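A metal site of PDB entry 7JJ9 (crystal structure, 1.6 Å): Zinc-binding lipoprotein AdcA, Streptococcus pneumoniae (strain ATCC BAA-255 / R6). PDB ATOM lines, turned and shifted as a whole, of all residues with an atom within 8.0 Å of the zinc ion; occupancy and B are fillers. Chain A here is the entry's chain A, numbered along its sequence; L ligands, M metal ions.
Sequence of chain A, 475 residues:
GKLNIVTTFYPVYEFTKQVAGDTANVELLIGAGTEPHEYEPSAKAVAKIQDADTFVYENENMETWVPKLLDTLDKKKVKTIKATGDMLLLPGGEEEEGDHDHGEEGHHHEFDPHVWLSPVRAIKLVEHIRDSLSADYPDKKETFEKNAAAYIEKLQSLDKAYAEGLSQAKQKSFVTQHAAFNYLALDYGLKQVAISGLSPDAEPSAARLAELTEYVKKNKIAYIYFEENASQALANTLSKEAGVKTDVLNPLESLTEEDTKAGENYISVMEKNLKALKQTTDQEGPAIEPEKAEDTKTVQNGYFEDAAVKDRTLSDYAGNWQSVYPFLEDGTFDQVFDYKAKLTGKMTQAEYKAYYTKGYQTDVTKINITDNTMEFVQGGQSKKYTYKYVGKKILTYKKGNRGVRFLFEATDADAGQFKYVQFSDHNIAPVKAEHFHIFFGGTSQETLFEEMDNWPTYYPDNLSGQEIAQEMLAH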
ATOM      1  N   GLN A 300      12.802   9.672  -0.586  1.00  0.00           N
ATOM      2  CA  GLN A 300      12.312   9.119   0.671  1.00  0.00           C
ATOM      3  C   GLN A 300      13.442   8.585   1.522  1.00  0.00           C
ATOM      4  O   GLN A 300      13.365   8.625   2.760  1.00  0.00           O
ATOM      5  CB  GLN A 300      11.267   8.051   0.389  1.00  0.00           C
ATOM      6  CG  GLN A 300       9.958   8.645  -0.097  1.00  0.00           C
ATOM      7  CD  GLN A 300       8.829   7.647  -0.068  1.00  0.00           C
ATOM      8  OE1 GLN A 300       9.050   6.430  -0.154  1.00  0.00           O
ATOM      9  NE2 GLN A 300       7.601   8.149   0.069  1.00  0.00           N
ATOM     10  N   TYR A 360      10.120   5.433  20.009  1.00  0.00           N
ATOM     11  CA  TYR A 360       8.691   5.517  19.932  1.00  0.00           C
ATOM     12  C   TYR A 360       8.020   5.911  21.226  1.00  0.00           C
ATOM     13  O   TYR A 360       6.829   6.249  21.200  1.00  0.00           O
ATOM     14  CB  TYR A 360       8.126   4.164  19.525  1.00  0.00           C
ATOM     15  CG  TYR A 360       8.430   3.695  18.115  1.00  0.00           C
ATOM     16  CD1 TYR A 360       8.766   4.579  17.103  1.00  0.00           C
ATOM     17  CD2 TYR A 360       8.397   2.334  17.811  1.00  0.00           C
ATOM     18  CE1 TYR A 360       9.022   4.120  15.808  1.00  0.00           C
ATOM     19  CE2 TYR A 360       8.671   1.877  16.532  1.00  0.00           C
ATOM     20  CZ  TYR A 360       8.981   2.768  15.537  1.00  0.00           C
ATOM     21  OH  TYR A 360       9.233   2.273  14.274  1.00  0.00           O
ATOM     22  N   SER A 424       8.501  15.000  10.644  1.00  0.00           N
ATOM     23  CA  SER A 424       9.363  14.333   9.681  1.00  0.00           C
ATOM     24  C   SER A 424       8.613  13.154   9.087  1.00  0.00           C
ATOM     25  O   SER A 424       8.121  12.300   9.834  1.00  0.00           O
ATOM     26  CB  SER A 424      10.666  13.850  10.338  1.00  0.00           C
ATOM     27  OG  SER A 424      11.388  13.012   9.453  1.00  0.00           O
ATOM     28  N   ASP A 425       8.507  13.132   7.765  1.00  0.00           N
ATOM     29  CA  ASP A 425       7.725  12.100   7.101  1.00  0.00           C
ATOM     30  C   ASP A 425       8.333  11.608   5.800  1.00  0.00           C
ATOM     31  O   ASP A 425       7.639  10.967   5.001  1.00  0.00           O
ATOM     32  CB  ASP A 425       6.299  12.614   6.853  1.00  0.00           C
ATOM     33  CG  ASP A 425       6.206  13.499   5.648  1.00  0.00           C
ATOM     34  OD1 ASP A 425       7.197  14.218   5.322  1.00  0.00           O
ATOM     35  OD2 ASP A 425       5.123  13.530   5.017  1.00  0.00           O
ATOM     36  N   HIS A 426       9.633  11.855   5.571  1.00  0.00           N
ATOM     37  CA  HIS A 426      10.380  11.422   4.391  1.00  0.00           C
ATOM     38  C   HIS A 426       9.981  12.146   3.119  1.00  0.00           C
ATOM     39  O   HIS A 426      10.493  11.840   2.047  1.00  0.00           O
ATOM     40  CB  HIS A 426      10.267   9.899   4.227  1.00  0.00           C
ATOM     41  CG  HIS A 426      10.448   9.191   5.529  1.00  0.00           C
ATOM     42  ND1 HIS A 426      11.649   9.168   6.179  1.00  0.00           N
ATOM     43  CD2 HIS A 426       9.547   8.618   6.364  1.00  0.00           C
ATOM     44  CE1 HIS A 426      11.516   8.554   7.340  1.00  0.00           C
ATOM     45  NE2 HIS A 426      10.242   8.228   7.491  1.00  0.00           N
ATOM     46  N   HIS A 435       2.744   8.511   7.150  1.00  0.00           N
ATOM     47  CA  HIS A 435       3.043   8.359   8.557  1.00  0.00           C
ATOM     48  C   HIS A 435       3.967   9.495   8.921  1.00  0.00           C
ATOM     49  O   HIS A 435       4.475  10.197   8.039  1.00  0.00           O
ATOM     50  CB  HIS A 435       3.672   6.991   8.881  1.00  0.00           C
ATOM     51  CG  HIS A 435       5.120   6.872   8.513  1.00  0.00           C
ATOM     52  ND1 HIS A 435       5.557   6.345   7.315  1.00  0.00           N
ATOM     53  CD2 HIS A 435       6.237   7.206   9.204  1.00  0.00           C
ATOM     54  CE1 HIS A 435       6.883   6.379   7.282  1.00  0.00           C
ATOM     55  NE2 HIS A 435       7.313   6.881   8.422  1.00  0.00           N
ATOM     56  N   PHE A 436       4.151   9.733  10.205  1.00  0.00           N
ATOM     57  CA  PHE A 436       5.127  10.752  10.545  1.00  0.00           C
ATOM     58  C   PHE A 436       5.804  10.455  11.864  1.00  0.00           C
ATOM     59  O   PHE A 436       5.321   9.696  12.693  1.00  0.00           O
ATOM     60  CB  PHE A 436       4.493  12.160  10.551  1.00  0.00           C
ATOM     61  CG  PHE A 436       3.351  12.350  11.505  1.00  0.00           C
ATOM     62  CD1 PHE A 436       3.558  12.554  12.859  1.00  0.00           C
ATOM     63  CD2 PHE A 436       2.045  12.424  11.019  1.00  0.00           C
ATOM     64  CE1 PHE A 436       2.498  12.759  13.731  1.00  0.00           C
ATOM     65  CE2 PHE A 436       0.992  12.643  11.883  1.00  0.00           C
ATOM     66  CZ  PHE A 436       1.189  12.806  13.233  1.00  0.00           C
ATOM     67  N   HIS A 437       6.956  11.069  12.019  1.00  0.00           N
ATOM     68  CA  HIS A 437       7.676  11.170  13.276  1.00  0.00           C
ATOM     69  C   HIS A 437       7.562  12.606  13.752  1.00  0.00           C
ATOM     70  O   HIS A 437       7.829  13.534  12.982  1.00  0.00           O
ATOM     71  CB  HIS A 437       9.140  10.756  13.067  1.00  0.00           C
ATOM     72  CG  HIS A 437       9.284   9.533  12.207  1.00  0.00           C
ATOM     73  ND1 HIS A 437       9.146   8.259  12.724  1.00  0.00           N
ATOM     74  CD2 HIS A 437       9.472   9.374  10.879  1.00  0.00           C
ATOM     75  CE1 HIS A 437       9.253   7.374  11.761  1.00  0.00           C
ATOM     76  NE2 HIS A 437       9.435   8.017  10.615  1.00  0.00           N
ATOM     77  N   TRP A 455      11.376  10.057  19.072  1.00  0.00           N
ATOM     78  CA  TRP A 455      10.673  10.527  17.867  1.00  0.00           C
ATOM     79  C   TRP A 455       9.347   9.780  17.791  1.00  0.00           C
ATOM     80  O   TRP A 455       9.163   8.874  16.960  1.00  0.00           O
ATOM     81  CB  TRP A 455      11.522  10.316  16.605  1.00  0.00           C
ATOM     82  CG  TRP A 455      12.725   9.450  16.770  1.00  0.00           C
ATOM     83  CD1 TRP A 455      13.974   9.869  17.108  1.00  0.00           C
ATOM     84  CD2 TRP A 455      12.815   8.021  16.604  1.00  0.00           C
ATOM     85  NE1 TRP A 455      14.835   8.808  17.170  1.00  0.00           N
ATOM     86  CE2 TRP A 455      14.152   7.653  16.873  1.00  0.00           C
ATOM     87  CE3 TRP A 455      11.896   7.024  16.272  1.00  0.00           C
ATOM     88  CZ2 TRP A 455      14.588   6.343  16.807  1.00  0.00           C
ATOM     89  CZ3 TRP A 455      12.343   5.702  16.206  1.00  0.00           C
ATOM     90  CH2 TRP A 455      13.673   5.382  16.467  1.00  0.00           C
ATOM     91  N   THR A 457       5.990   8.254  16.863  1.00  0.00           N
ATOM     92  CA  THR A 457       5.723   7.866  15.493  1.00  0.00           C
ATOM     93  C   THR A 457       4.259   7.450  15.360  1.00  0.00           C
ATOM     94  O   THR A 457       3.734   6.715  16.197  1.00  0.00           O
ATOM     95  CB  THR A 457       6.643   6.728  15.068  1.00  0.00           C
ATOM     96  OG1 THR A 457       7.984   7.252  15.047  1.00  0.00           O
ATOM     97  CG2 THR A 457       6.377   6.215  13.683  1.00  0.00           C
ATOM     98  N   TYR A 458       3.627   7.938  14.290  1.00  0.00           N
ATOM     99  CA  TYR A 458       2.175   7.882  14.140  1.00  0.00           C
ATOM    100  C   TYR A 458       1.817   7.385  12.746  1.00  0.00           C
ATOM    101  O   TYR A 458       2.366   7.835  11.750  1.00  0.00           O
ATOM    102  CB  TYR A 458       1.536   9.276  14.399  1.00  0.00           C
ATOM    103  CG  TYR A 458       1.703   9.657  15.839  1.00  0.00           C
ATOM    104  CD1 TYR A 458       2.891  10.193  16.279  1.00  0.00           C
ATOM    105  CD2 TYR A 458       0.706   9.404  16.776  1.00  0.00           C
ATOM    106  CE1 TYR A 458       3.092  10.455  17.605  1.00  0.00           C
ATOM    107  CE2 TYR A 458       0.896   9.688  18.105  1.00  0.00           C
ATOM    108  CZ  TYR A 458       2.103  10.203  18.513  1.00  0.00           C
ATOM    109  OH  TYR A 458       2.333  10.476  19.855  1.00  0.00           O
ATOM    110  N   TYR A 459       0.834   6.478  12.701  1.00  0.00           N
ATOM    111  CA  TYR A 459       0.232   5.973  11.472  1.00  0.00           C
ATOM    112  C   TYR A 459      -1.272   6.231  11.522  1.00  0.00           C
ATOM    113  O   TYR A 459      -1.805   6.549  12.574  1.00  0.00           O
ATOM    114  CB  TYR A 459       0.493   4.476  11.309  1.00  0.00           C
ATOM    115  CG  TYR A 459       1.847   4.135  10.726  1.00  0.00           C
ATOM    116  CD1 TYR A 459       3.015   4.333  11.457  1.00  0.00           C
ATOM    117  CD2 TYR A 459       1.958   3.635   9.419  1.00  0.00           C
ATOM    118  CE1 TYR A 459       4.250   4.047  10.911  1.00  0.00           C
ATOM    119  CE2 TYR A 459       3.224   3.337   8.865  1.00  0.00           C
ATOM    120  CZ  TYR A 459       4.339   3.550   9.629  1.00  0.00           C
ATOM    121  OH  TYR A 459       5.609   3.279   9.135  1.00  0.00           O
ATOM    122  N   MET A 472       5.593  -0.928   7.663  1.00  0.00           N
ATOM    123  CA  MET A 472       6.954  -0.546   8.026  1.00  0.00           C
ATOM    124  C   MET A 472       8.007  -1.240   7.187  1.00  0.00           C
ATOM    125  O   MET A 472       9.123  -0.745   7.053  1.00  0.00           O
ATOM    126  CB  MET A 472       7.208  -0.876   9.498  1.00  0.00           C
ATOM    127  CG  MET A 472       6.637   0.120  10.452  1.00  0.00           C
ATOM    128  SD  MET A 472       6.959  -0.322  12.153  1.00  0.00           S
ATOM    129  CE  MET A 472       6.317   1.163  12.951  1.00  0.00           C
ATOM    130  N   HIS A 475       8.301  -0.831   0.698  1.00  0.00           N
ATOM    131  CA  HIS A 475       9.237   0.099   0.041  1.00  0.00           C
ATOM    132  C   HIS A 475      10.617  -0.544  -0.073  1.00  0.00           C
ATOM    133  O   HIS A 475      10.824  -1.503  -0.828  1.00  0.00           O
ATOM    134  CB  HIS A 475       9.353   1.448   0.790  1.00  0.00           C
ATOM    135  CG  HIS A 475       8.063   1.937   1.394  1.00  0.00           C
ATOM    136  ND1 HIS A 475       7.980   2.408   2.683  1.00  0.00           N
ATOM    137  CD2 HIS A 475       6.804   1.992   0.887  1.00  0.00           C
ATOM    138  CE1 HIS A 475       6.726   2.733   2.952  1.00  0.00           C
ATOM    139  NE2 HIS A 475       5.998   2.497   1.875  1.00  0.00           N
HETATM  140 CL1  LIG L   1      10.380   5.181   8.923  1.00  0.00          CL
HETATM  141 ZN    ZN M   1       9.361   7.101   8.866  1.00  0.00          ZN
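The nearest printed residue that does not touch the zinc ion is Tyr 459 (5.4 Å).
The zinc ion is bound by NE2 of His 437 (2.0 Å).
NE2 of His 426 is bound to the zinc ion, at 2.0 Å.
The zinc ion is bound by NE2 of His 435.
The zinc ion is bound by CL1 of the ligand (2.2 Å).
The zinc ion has four donor atoms within binding distance.
The backbone NH of His 437 is in hydrogen-bond range of the backbone carbonyl oxygen of Ser 424 (2.8 Å).
A ring nitrogen (ND1) of His 437 is in hydrogen-bond range of the side-chain hydroxyl of Thr 457 (2.8 Å).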
